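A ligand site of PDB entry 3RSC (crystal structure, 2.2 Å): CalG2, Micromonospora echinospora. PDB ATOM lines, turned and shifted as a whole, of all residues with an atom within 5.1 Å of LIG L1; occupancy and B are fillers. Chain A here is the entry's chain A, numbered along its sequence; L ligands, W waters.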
ATOM      1  N   HIS A  31       2.142  14.783  32.976  1.00  0.00           N
ATOM      2  CA  HIS A  31       1.230  13.636  33.045  1.00  0.00           C
ATOM      3  C   HIS A  31       1.905  12.391  33.608  1.00  0.00           C
ATOM      4  O   HIS A  31       1.448  11.816  34.602  1.00  0.00           O
ATOM      5  CB  HIS A  31       0.638  13.321  31.664  1.00  0.00           C
ATOM      6  CG  HIS A  31      -0.447  14.266  31.239  1.00  0.00           C
ATOM      7  ND1 HIS A  31      -0.180  15.510  30.695  1.00  0.00           N
ATOM      8  CD2 HIS A  31      -1.793  14.158  31.299  1.00  0.00           C
ATOM      9  CE1 HIS A  31      -1.320  16.118  30.417  1.00  0.00           C
ATOM     10  NE2 HIS A  31      -2.318  15.317  30.770  1.00  0.00           N
ATOM     11  N   GLY A  32       2.981  11.959  32.961  1.00  0.00           N
ATOM     12  CA  GLY A  32       3.663  10.742  33.359  1.00  0.00           C
ATOM     13  C   GLY A  32       4.083  10.722  34.812  1.00  0.00           C
ATOM     14  O   GLY A  32       4.136   9.661  35.441  1.00  0.00           O
ATOM     15  N   LEU A  35       0.127  11.040  37.226  1.00  0.00           N
ATOM     16  CA  LEU A  35      -0.859   9.962  37.180  1.00  0.00           C
ATOM     17  C   LEU A  35      -0.593   8.763  38.116  1.00  0.00           C
ATOM     18  O   LEU A  35      -1.511   8.291  38.777  1.00  0.00           O
ATOM     19  CB  LEU A  35      -1.091   9.481  35.743  1.00  0.00           C
ATOM     20  CG  LEU A  35      -1.725  10.502  34.795  1.00  0.00           C
ATOM     21  CD1 LEU A  35      -2.165   9.840  33.495  1.00  0.00           C
ATOM     22  CD2 LEU A  35      -2.890  11.195  35.460  1.00  0.00           C
ATOM     23  N   ARG A 234      -9.801   7.051  35.815  1.00  0.00           N
ATOM     24  CA  ARG A 234      -9.292   8.282  35.226  1.00  0.00           C
ATOM     25  C   ARG A 234     -10.306   8.901  34.273  1.00  0.00           C
ATOM     26  O   ARG A 234     -10.045   9.043  33.067  1.00  0.00           O
ATOM     27  CB  ARG A 234      -7.972   8.021  34.506  1.00  0.00           C
ATOM     28  CG  ARG A 234      -6.909   7.475  35.429  1.00  0.00           C
ATOM     29  CD  ARG A 234      -5.649   7.097  34.689  1.00  0.00           C
ATOM     30  NE  ARG A 234      -4.545   6.941  35.632  1.00  0.00           N
ATOM     31  CZ  ARG A 234      -3.380   6.375  35.330  1.00  0.00           C
ATOM     32  NH1 ARG A 234      -3.175   5.893  34.112  1.00  0.00           N
ATOM     33  NH2 ARG A 234      -2.431   6.287  36.250  1.00  0.00           N
ATOM     34  N   LEU A 237      -9.729  12.040  31.919  1.00  0.00           N
ATOM     35  CA  LEU A 237      -9.111  11.914  30.604  1.00  0.00           C
ATOM     36  C   LEU A 237     -10.155  11.551  29.552  1.00  0.00           C
ATOM     37  O   LEU A 237      -9.814  11.073  28.466  1.00  0.00           O
ATOM     38  CB  LEU A 237      -8.001  10.871  30.621  1.00  0.00           C
ATOM     39  CG  LEU A 237      -6.792  11.168  31.500  1.00  0.00           C
ATOM     40  CD1 LEU A 237      -5.853   9.962  31.543  1.00  0.00           C
ATOM     41  CD2 LEU A 237      -6.060  12.407  31.024  1.00  0.00           C
ATOM     42  N   SER A 253      -0.250   5.248  20.329  1.00  0.00           N
ATOM     43  CA  SER A 253       0.004   6.535  20.959  1.00  0.00           C
ATOM     44  C   SER A 253       1.488   6.892  20.945  1.00  0.00           C
ATOM     45  O   SER A 253       2.340   6.016  21.067  1.00  0.00           O
ATOM     46  CB  SER A 253      -0.504   6.512  22.409  1.00  0.00           C
ATOM     47  OG  SER A 253      -0.450   7.807  22.993  1.00  0.00           O
ATOM     48  N   LEU A 254       1.775   8.178  20.777  1.00  0.00           N
ATOM     49  CA  LEU A 254       3.143   8.675  20.907  1.00  0.00           C
ATOM     50  C   LEU A 254       3.323   9.391  22.238  1.00  0.00           C
ATOM     51  O   LEU A 254       4.334  10.065  22.463  1.00  0.00           O
ATOM     52  CB  LEU A 254       3.518   9.615  19.756  1.00  0.00           C
ATOM     53  CG  LEU A 254       3.740   8.950  18.405  1.00  0.00           C
ATOM     54  CD1 LEU A 254       4.286   9.945  17.391  1.00  0.00           C
ATOM     55  CD2 LEU A 254       4.684   7.759  18.529  1.00  0.00           C
ATOM     56  N   GLY A 255       2.336   9.241  23.117  1.00  0.00           N
ATOM     57  CA  GLY A 255       2.396   9.854  24.432  1.00  0.00           C
ATOM     58  C   GLY A 255       2.010  11.323  24.444  1.00  0.00           C
ATOM     59  O   GLY A 255       1.184  11.761  23.639  1.00  0.00           O
ATOM     60  N   THR A 256       2.603  12.074  25.363  1.00  0.00           N
ATOM     61  CA  THR A 256       2.210  13.454  25.610  1.00  0.00           C
ATOM     62  C   THR A 256       3.358  14.433  25.443  1.00  0.00           C
ATOM     63  O   THR A 256       3.185  15.634  25.635  1.00  0.00           O
ATOM     64  CB  THR A 256       1.663  13.623  27.044  1.00  0.00           C
ATOM     65  OG1 THR A 256       2.731  13.418  27.984  1.00  0.00           O
ATOM     66  CG2 THR A 256       0.555  12.625  27.325  1.00  0.00           C
ATOM     67  N   THR A 257       4.528  13.937  25.070  1.00  0.00           N
ATOM     68  CA  THR A 257       5.744  14.736  25.108  1.00  0.00           C
ATOM     69  C   THR A 257       6.366  15.033  23.741  1.00  0.00           C
ATOM     70  O   THR A 257       6.555  16.205  23.387  1.00  0.00           O
ATOM     71  CB  THR A 257       6.804  14.118  26.060  1.00  0.00           C
ATOM     72  OG1 THR A 257       6.185  13.789  27.313  1.00  0.00           O
ATOM     73  CG2 THR A 257       7.946  15.087  26.304  1.00  0.00           C
ATOM     74  N   THR A 282      -4.310   8.014  20.159  1.00  0.00           N
ATOM     75  CA  THR A 282      -4.372   9.165  21.053  1.00  0.00           C
ATOM     76  C   THR A 282      -3.231  10.147  20.754  1.00  0.00           C
ATOM     77  O   THR A 282      -2.077   9.748  20.551  1.00  0.00           O
ATOM     78  CB  THR A 282      -4.343   8.751  22.535  1.00  0.00           C
ATOM     79  OG1 THR A 282      -3.070   8.209  22.866  1.00  0.00           O
ATOM     80  CG2 THR A 282      -5.427   7.709  22.809  1.00  0.00           C
ATOM     81  N   LEU A 283      -3.568  11.426  20.729  1.00  0.00           N
ATOM     82  CA  LEU A 283      -2.669  12.470  20.241  1.00  0.00           C
ATOM     83  C   LEU A 283      -1.987  13.262  21.356  1.00  0.00           C
ATOM     84  O   LEU A 283      -0.943  13.876  21.131  1.00  0.00           O
ATOM     85  CB  LEU A 283      -3.436  13.397  19.300  1.00  0.00           C
ATOM     86  CG  LEU A 283      -4.108  12.683  18.123  1.00  0.00           C
ATOM     87  CD1 LEU A 283      -4.979  13.634  17.310  1.00  0.00           C
ATOM     88  CD2 LEU A 283      -3.056  12.034  17.230  1.00  0.00           C
ATOM     89  N   GLY A 284      -2.564  13.250  22.545  1.00  0.00           N
ATOM     90  CA  GLY A 284      -1.930  13.869  23.698  1.00  0.00           C
ATOM     91  C   GLY A 284      -1.847  15.377  23.664  1.00  0.00           C
ATOM     92  O   GLY A 284      -0.792  15.961  23.960  1.00  0.00           O
ATOM     93  N   ARG A 303      -7.783  13.419  21.171  1.00  0.00           N
ATOM     94  CA  ARG A 303      -6.799  14.199  21.878  1.00  0.00           C
ATOM     95  C   ARG A 303      -6.424  13.449  23.149  1.00  0.00           C
ATOM     96  O   ARG A 303      -5.251  13.303  23.471  1.00  0.00           O
ATOM     97  CB  ARG A 303      -7.347  15.589  22.212  1.00  0.00           C
ATOM     98  CG  ARG A 303      -7.757  16.390  20.982  1.00  0.00           C
ATOM     99  CD  ARG A 303      -8.268  17.777  21.338  1.00  0.00           C
ATOM    100  NE  ARG A 303      -8.621  18.533  20.145  1.00  0.00           N
ATOM    101  CZ  ARG A 303      -7.769  19.273  19.444  1.00  0.00           C
ATOM    102  NH1 ARG A 303      -6.502  19.373  19.823  1.00  0.00           N
ATOM    103  NH2 ARG A 303      -8.188  19.925  18.366  1.00  0.00           N
ATOM    104  N   TRP A 304      -7.445  12.950  23.853  1.00  0.00           N
ATOM    105  CA  TRP A 304      -7.229  12.180  25.067  1.00  0.00           C
ATOM    106  C   TRP A 304      -8.327  11.126  25.263  1.00  0.00           C
ATOM    107  O   TRP A 304      -9.510  11.423  25.121  1.00  0.00           O
ATOM    108  CB  TRP A 304      -7.220  13.085  26.309  1.00  0.00           C
ATOM    109  CG  TRP A 304      -6.222  14.206  26.272  1.00  0.00           C
ATOM    110  CD1 TRP A 304      -6.451  15.497  25.874  1.00  0.00           C
ATOM    111  CD2 TRP A 304      -4.849  14.153  26.684  1.00  0.00           C
ATOM    112  NE1 TRP A 304      -5.300  16.233  25.997  1.00  0.00           N
ATOM    113  CE2 TRP A 304      -4.298  15.440  26.486  1.00  0.00           C
ATOM    114  CE3 TRP A 304      -4.027  13.134  27.189  1.00  0.00           C
ATOM    115  CZ2 TRP A 304      -2.973  15.738  26.774  1.00  0.00           C
ATOM    116  CZ3 TRP A 304      -2.698  13.441  27.476  1.00  0.00           C
ATOM    117  CH2 TRP A 304      -2.191  14.735  27.268  1.00  0.00           C
ATOM    118  N   VAL A 305      -7.912   9.899  25.558  1.00  0.00           N
ATOM    119  CA  VAL A 305      -8.785   8.898  26.165  1.00  0.00           C
ATOM    120  C   VAL A 305      -7.965   8.082  27.158  1.00  0.00           C
ATOM    121  O   VAL A 305      -6.765   7.882  26.949  1.00  0.00           O
ATOM    122  CB  VAL A 305      -9.452   7.942  25.145  1.00  0.00           C
ATOM    123  CG1 VAL A 305     -10.297   8.712  24.137  1.00  0.00           C
ATOM    124  CG2 VAL A 305      -8.410   7.081  24.433  1.00  0.00           C
ATOM    125  N   PRO A 306      -8.593   7.624  28.245  1.00  0.00           N
ATOM    126  CA  PRO A 306      -7.853   6.833  29.236  1.00  0.00           C
ATOM    127  C   PRO A 306      -7.244   5.588  28.593  1.00  0.00           C
ATOM    128  O   PRO A 306      -7.984   4.729  28.116  1.00  0.00           O
ATOM    129  CB  PRO A 306      -8.935   6.416  30.234  1.00  0.00           C
ATOM    130  CG  PRO A 306     -10.023   7.416  30.067  1.00  0.00           C
ATOM    131  CD  PRO A 306     -10.012   7.781  28.615  1.00  0.00           C
ATOM    132  N   HIS A 307      -5.920   5.502  28.585  1.00  0.00           N
ATOM    133  CA  HIS A 307      -5.242   4.333  28.031  1.00  0.00           C
ATOM    134  C   HIS A 307      -5.614   3.053  28.772  1.00  0.00           C
ATOM    135  O   HIS A 307      -5.645   1.978  28.189  1.00  0.00           O
ATOM    136  CB  HIS A 307      -3.725   4.525  28.057  1.00  0.00           C
ATOM    137  CG  HIS A 307      -3.222   5.435  26.978  1.00  0.00           C
ATOM    138  ND1 HIS A 307      -1.876   5.687  26.788  1.00  0.00           N
ATOM    139  CD2 HIS A 307      -3.870   6.156  26.037  1.00  0.00           C
ATOM    140  CE1 HIS A 307      -1.722   6.516  25.778  1.00  0.00           C
ATOM    141  NE2 HIS A 307      -2.917   6.815  25.300  1.00  0.00           N
ATOM    142  N   THR A 319       3.091   1.853  21.397  1.00  0.00           N
ATOM    143  CA  THR A 319       3.450   3.007  22.205  1.00  0.00           C
ATOM    144  C   THR A 319       4.878   3.444  21.899  1.00  0.00           C
ATOM    145  O   THR A 319       5.708   2.625  21.493  1.00  0.00           O
ATOM    146  CB  THR A 319       3.306   2.695  23.709  1.00  0.00           C
ATOM    147  OG1 THR A 319       3.727   3.830  24.482  1.00  0.00           O
ATOM    148  CG2 THR A 319       4.161   1.497  24.088  1.00  0.00           C
ATOM    149  N   HIS A 320       5.171   4.723  22.099  1.00  0.00           N
ATOM    150  CA  HIS A 320       6.531   5.221  21.912  1.00  0.00           C
ATOM    151  C   HIS A 320       7.463   4.670  22.998  1.00  0.00           C
ATOM    152  O   HIS A 320       8.670   4.577  22.800  1.00  0.00           O
ATOM    153  CB  HIS A 320       6.545   6.743  21.936  1.00  0.00           C
ATOM    154  CG  HIS A 320       6.128   7.328  23.246  1.00  0.00           C
ATOM    155  ND1 HIS A 320       4.919   7.014  23.845  1.00  0.00           N
ATOM    156  CD2 HIS A 320       6.744   8.194  24.081  1.00  0.00           C
ATOM    157  CE1 HIS A 320       4.813   7.677  24.984  1.00  0.00           C
ATOM    158  NE2 HIS A 320       5.910   8.397  25.150  1.00  0.00           N
ATOM    159  N   GLY A 322       6.637   5.412  26.664  1.00  0.00           N
ATOM    160  CA  GLY A 322       6.372   6.079  27.932  1.00  0.00           C
ATOM    161  C   GLY A 322       6.101   5.055  29.016  1.00  0.00           C
ATOM    162  O   GLY A 322       5.340   4.115  28.798  1.00  0.00           O
ATOM    163  N   MET A 323       6.715   5.213  30.182  1.00  0.00           N
ATOM    164  CA  MET A 323       6.632   4.165  31.202  1.00  0.00           C
ATOM    165  C   MET A 323       5.201   3.894  31.647  1.00  0.00           C
ATOM    166  O   MET A 323       4.819   2.742  31.860  1.00  0.00           O
ATOM    167  CB  MET A 323       7.507   4.473  32.415  1.00  0.00           C
ATOM    168  CG  MET A 323       7.512   3.330  33.422  1.00  0.00           C
ATOM    169  SD  MET A 323       8.546   1.806  32.737  1.00  0.00           S
ATOM    170  CE  MET A 323      10.307   2.426  33.322  1.00  0.00           C
ATOM    171  N   GLY A 324       4.418   4.957  31.781  1.00  0.00           N
ATOM    172  CA  GLY A 324       3.039   4.814  32.187  1.00  0.00           C
ATOM    173  C   GLY A 324       2.287   3.879  31.248  1.00  0.00           C
ATOM    174  O   GLY A 324       1.706   2.888  31.686  1.00  0.00           O
ATOM    175  N   THR A 325       2.317   4.194  29.966  1.00  0.00           N
ATOM    176  CA  THR A 325       1.623   3.384  28.977  1.00  0.00           C
ATOM    177  C   THR A 325       2.137   1.943  28.926  1.00  0.00           C
ATOM    178  O   THR A 325       1.351   1.006  28.878  1.00  0.00           O
ATOM    179  CB  THR A 325       1.655   4.008  27.579  1.00  0.00           C
ATOM    180  OG1 THR A 325       0.875   5.213  27.592  1.00  0.00           O
ATOM    181  CG2 THR A 325       1.072   3.046  26.550  1.00  0.00           C
ATOM    182  N   GLU A 328       0.752   0.188  32.002  1.00  0.00           N
ATOM    183  CA  GLU A 328      -0.691  -0.009  31.918  1.00  0.00           C
ATOM    184  C   GLU A 328      -0.991  -1.137  30.933  1.00  0.00           C
ATOM    185  O   GLU A 328      -1.937  -1.908  31.121  1.00  0.00           O
ATOM    186  CB  GLU A 328      -1.387   1.290  31.494  1.00  0.00           C
ATOM    187  CG  GLU A 328      -1.194   2.414  32.514  1.00  0.00           C
ATOM    188  CD  GLU A 328      -1.460   3.806  31.953  1.00  0.00           C
ATOM    189  OE1 GLU A 328      -1.140   4.793  32.642  1.00  0.00           O
ATOM    190  OE2 GLU A 328      -1.997   3.915  30.827  1.00  0.00           O
ATOM    191  N   ASP A 344      14.140  10.079  25.837  1.00  0.00           N
ATOM    192  CA  ASP A 344      13.591   9.835  27.168  1.00  0.00           C
ATOM    193  C   ASP A 344      12.982   8.440  27.335  1.00  0.00           C
ATOM    194  O   ASP A 344      12.830   7.969  28.456  1.00  0.00           O
ATOM    195  CB  ASP A 344      12.562  10.905  27.533  1.00  0.00           C
ATOM    196  CG  ASP A 344      11.409  10.980  26.537  1.00  0.00           C
ATOM    197  OD1 ASP A 344      11.626  10.712  25.331  1.00  0.00           O
ATOM    198  OD2 ASP A 344      10.288  11.315  26.957  1.00  0.00           O
ATOM    199  N   VAL A 345      12.631   7.797  26.229  1.00  0.00           N
ATOM    200  CA  VAL A 345      12.051   6.456  26.268  1.00  0.00           C
ATOM    201  C   VAL A 345      12.941   5.386  25.658  1.00  0.00           C
ATOM    202  O   VAL A 345      12.551   4.225  25.575  1.00  0.00           O
ATOM    203  CB  VAL A 345      10.682   6.408  25.555  1.00  0.00           C
ATOM    204  CG1 VAL A 345       9.682   7.315  26.258  1.00  0.00           C
ATOM    205  CG2 VAL A 345      10.840   6.783  24.081  1.00  0.00           C
HETATM  206  P1  LIG L   1       2.759   8.196  28.198  1.00  0.00           P
HETATM  207  O1  LIG L   1       3.471   7.402  29.267  1.00  0.00           O
HETATM  208  O2  LIG L   1       2.005   7.450  27.121  1.00  0.00           O
HETATM  209  O3  LIG L   1       3.732   9.228  27.435  1.00  0.00           O
HETATM  210  P2  LIG L   1       4.836  10.224  28.079  1.00  0.00           P
HETATM  211  O4  LIG L   1       4.632  10.201  29.572  1.00  0.00           O
HETATM  212  O5  LIG L   1       6.149   9.655  27.599  1.00  0.00           O
HETATM  213  O6  LIG L   1       4.473  11.531  27.425  1.00  0.00           O
HETATM  214  O7  LIG L   1       1.697   9.186  28.907  1.00  0.00           O
HETATM  215  C1  LIG L   1       1.745   9.385  30.318  1.00  0.00           C
HETATM  216  C2  LIG L   1       0.427   8.990  30.949  1.00  0.00           C
HETATM  217  O8  LIG L   1      -0.660   9.595  30.239  1.00  0.00           O
HETATM  218  C3  LIG L   1       0.231   7.478  30.854  1.00  0.00           C
HETATM  219  O9  LIG L   1      -0.192   6.998  32.130  1.00  0.00           O
HETATM  220  C4  LIG L   1      -0.880   7.269  29.832  1.00  0.00           C
HETATM  221  C5  LIG L   1      -1.635   8.589  29.914  1.00  0.00           C
HETATM  222  N1  LIG L   1      -2.344   8.941  28.680  1.00  0.00           N
HETATM  223  C6  LIG L   1      -3.726   8.659  28.549  1.00  0.00           C
HETATM  224  O10 LIG L   1      -4.332   8.068  29.474  1.00  0.00           O
HETATM  225  N2  LIG L   1      -4.406   8.986  27.440  1.00  0.00           N
HETATM  226  C7  LIG L   1      -3.785   9.607  26.430  1.00  0.00           C
HETATM  227  O11 LIG L   1      -4.433   9.914  25.396  1.00  0.00           O
HETATM  228  C8  LIG L   1      -2.345   9.928  26.539  1.00  0.00           C
HETATM  229  C9  LIG L   1      -1.633  10.632  25.418  1.00  0.00           C
HETATM  230  C10 LIG L   1      -1.675   9.577  27.700  1.00  0.00           C
HETATM  231  C1  LG2 L   2      18.290  17.126  34.232  1.00  0.00           C
HETATM  232  N1  LG2 L   2      16.985  15.130  34.544  1.00  0.00           N
HETATM  233  O1  LG2 L   2      18.734  17.059  35.360  1.00  0.00           O
HETATM  234  S1  LG2 L   2      13.332  19.933  32.135  1.00  0.00           S
HETATM  235  C2  LG2 L   2      17.201  16.230  33.834  1.00  0.00           C
HETATM  236  N2  LG2 L   2      10.423  12.750  29.804  1.00  0.00           N
HETATM  237  O2  LG2 L   2      14.787  15.475  34.832  1.00  0.00           O
HETATM  238  S2  LG2 L   2      13.494  21.083  30.494  1.00  0.00           S
HETATM  239  C3  LG2 L   2      16.477  16.514  32.766  1.00  0.00           C
HETATM  240  O3  LG2 L   2      15.651  13.583  35.788  1.00  0.00           O
HETATM  241  S3  LG2 L   2      11.793  21.025  29.447  1.00  0.00           S
HETATM  242  C4  LG2 L   2      16.606  17.836  32.153  1.00  0.00           C
HETATM  243  O4  LG2 L   2      18.051  19.626  31.557  1.00  0.00           O
HETATM  244  C5  LG2 L   2      18.043  18.256  31.967  1.00  0.00           C
HETATM  245  O5  LG2 L   2      14.354  16.046  31.651  1.00  0.00           O
HETATM  246  C6  LG2 L   2      18.857  18.125  33.254  1.00  0.00           C
HETATM  247  O6  LG2 L   2       9.640  12.716  28.823  1.00  0.00           O
HETATM  248  C7  LG2 L   2      15.784  14.803  35.017  1.00  0.00           C
HETATM  249  O7  LG2 L   2      12.916  15.370  29.942  1.00  0.00           O
HETATM  250  C8  LG2 L   2      14.373  12.972  35.974  1.00  0.00           C
HETATM  251  O8  LG2 L   2      12.929  14.353  33.455  1.00  0.00           O
HETATM  252  C9  LG2 L   2      18.628  17.450  30.889  1.00  0.00           C
HETATM  253  O9  LG2 L   2      10.225  13.734  32.563  1.00  0.00           O
HETATM  254  C10 LG2 L   2      18.957  16.668  30.065  1.00  0.00           C
HETATM  255  C11 LG2 L   2      19.077  15.558  29.190  1.00  0.00           C
HETATM  256  C12 LG2 L   2      18.188  14.565  29.246  1.00  0.00           C
HETATM  257  C13 LG2 L   2      17.123  14.621  30.200  1.00  0.00           C
HETATM  258  C14 LG2 L   2      16.371  14.913  31.057  1.00  0.00           C
HETATM  259  C15 LG2 L   2      15.569  15.488  32.148  1.00  0.00           C
HETATM  260  C16 LG2 L   2      15.638  18.677  31.759  1.00  0.00           C
HETATM  261  C17 LG2 L   2      14.163  18.401  31.886  1.00  0.00           C
HETATM  262  C18 LG2 L   2      11.879  19.751  28.236  1.00  0.00           C
HETATM  263  C19 LG2 L   2      13.484  15.016  31.199  1.00  0.00           C
HETATM  264  C20 LG2 L   2      12.372  14.791  32.219  1.00  0.00           C
HETATM  265  C21 LG2 L   2      11.378  13.736  31.723  1.00  0.00           C
HETATM  266  C22 LG2 L   2      10.947  14.014  30.289  1.00  0.00           C
HETATM  267  C23 LG2 L   2      12.154  14.306  29.393  1.00  0.00           C
HETATM  268  C24 LG2 L   2      11.707  14.681  27.986  1.00  0.00           C
HETATM  269  O   HOH W   1       8.427   9.785  29.070  1.00  0.00           O
HETATM  270  O   HOH W   2       4.970   7.862  31.367  1.00  0.00           O
HETATM  271  O   HOH W   3       7.882  10.976  25.869  1.00  0.00           O
HETATM  272  O   HOH W   4       2.167   5.935  24.532  1.00  0.00           O
HETATM  273  O   HOH W   5       1.219   7.474  34.353  1.00  0.00           O
HETATM  274  O   HOH W   6       6.726  10.687  31.608  1.00  0.00           O
HETATM  275  O   HOH W   7       4.189  12.725  30.547  1.00  0.00           O
HETATM  276  O   HOH W   8      -4.391   5.641  31.521  1.00  0.00           O
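An oxygen (O6) of LIG L1 is in hydrogen-bond range of the side-chain hydroxyl of Thr 256 (2.6 Å).
An oxygen (O6) of LIG L1 lies within hydrogen-bond range of the side-chain hydroxyl (OG1) of Thr 257, at 2.8 Å.
N2 of LIG L1 lies within hydrogen-bond range of O of Val 305 (2.7 Å).
A ring nitrogen (NE2) of His 307 lies close to a nitrogen (N2) of LIG L1 (3.4 Å).
The backbone NH (N) of Val 305 sits at hydrogen-bond distance from an oxygen (O11) of LIG L1 (3.5 Å).
The backbone NH (N) of Thr 257 sits at hydrogen-bond distance from an oxygen (O6) of LIG L1 (3.4 Å).
N of Thr 325 sits at hydrogen-bond distance from O1 of LIG L1, 3.5 Å away.
A ring nitrogen (NE2) of His 320 lies within hydrogen-bond range of an oxygen (O5) of LIG L1 (2.8 Å).
O9 of LIG L1 sits at hydrogen-bond distance from OE1 of Glu 328 (2.5 Å).
N of His 307 sits at hydrogen-bond distance from O10 of LIG L1, at 3.1 Å.
The side-chain carboxylate (OD2) of Asp 344 sits at hydrogen-bond distance from an oxygen (O6) of LG2 L2.
The backbone NH of Thr 256 is in hydrogen-bond range of an oxygen (O6) of LIG L1 (2.8 Å).
The side-chain hydroxyl (OG1) of Thr 325 sits at hydrogen-bond distance from an oxygen (O2) of LIG L1, 2.6 Å away.
The side-chain hydroxyl of Thr 282 lies close to an oxygen (O11) of LIG L1.
The side-chain hydroxyl of Thr 282 sits at hydrogen-bond distance from a ring nitrogen (NE2) of His 307, at 2.8 Å.
The backbone NH (N) of Gly 255 lies within hydrogen-bond range of the side-chain hydroxyl (OG) of Ser 253.
The backbone carbonyl oxygen of Leu 35 lies within hydrogen-bond range of the guanidinium group of Arg 234 (3.4 Å).
A ring nitrogen (ND1) of His 320 lies close to the backbone NH (N) of Gly 255, at 3.5 Å.
The side-chain carboxylate (OE1) of Glu 328 is in salt-bridge range of the guanidinium group (NH1) of Arg 234.
OG1 of Thr 325 lies within hydrogen-bond range of ND1 of His 307, at 2.9 Å.
The backbone NH (N) of Gly 284 sits at hydrogen-bond distance from the backbone carbonyl oxygen (O) of Arg 303, 2.8 Å away.
The side-chain hydroxyl (OG1) of Thr 319 is in hydrogen-bond range of a ring nitrogen (ND1) of His 320 (3.5 Å).
Merely in contact with LIG L1: Leu 237, Gly 255, Gly 322, Leu 35, Trp 304, Gly 324, Gly 284, Pro 306, Arg 234, Gly 32, Ser 253 and Arg 303.
Hydrophobic or aromatic side chains that line LIG L1: Leu 35, Leu 237, Trp 304, His 307 and His 320.
Within 4 Å of LIG L1: Gly 32, Leu 35, Arg 234, Leu 237, Ser 253, Gly 255, Thr 256, Thr 257, Thr 282, Gly 284, Arg 303, Trp 304, Val 305, Pro 306, His 307, His 320, Gly 322, Gly 324, Thr 325 and Glu 328.
The nearest printed residue that does not touch LIG L1 is Met 323 (4.02 Å).
Water W2 lies within hydrogen-bond range of O1 of LIG L1 (2.6 Å), N of Gly 324 (3.0 Å) and N of Met 323 (3.4 Å).
Water W1 lies within hydrogen-bond range of an oxygen (O5) of LIG L1, an oxygen (O6) of LG2 L2 and the side-chain carboxylate (OD2) of Asp 344.
Water W7 lies within hydrogen-bond range of an oxygen (O4) of LIG L1 (2.7 Å), the backbone NH (N) of Gly 32 (2.8 Å) and the side-chain hydroxyl (OG1) of Thr 256 (3.0 Å).
Water W3 lies within hydrogen-bond range of OD2 of Asp 344 (2.7 Å), O5 of LIG L1 (2.8 Å) and NE2 of His 320 (3.3 Å).
Water W4 lies within hydrogen-bond range of OG1 of Thr 319, O2 of LIG L1, ND1 of His 320, OG1 of Thr 325 and O of Ser 253.
Water W8 lies within hydrogen-bond range of NH1 of Arg 234 (2.9 Å), OE2 of Glu 328 (3.0 Å), O10 of LIG L1 (3.2 Å) and N of His 307 (3.3 Å).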
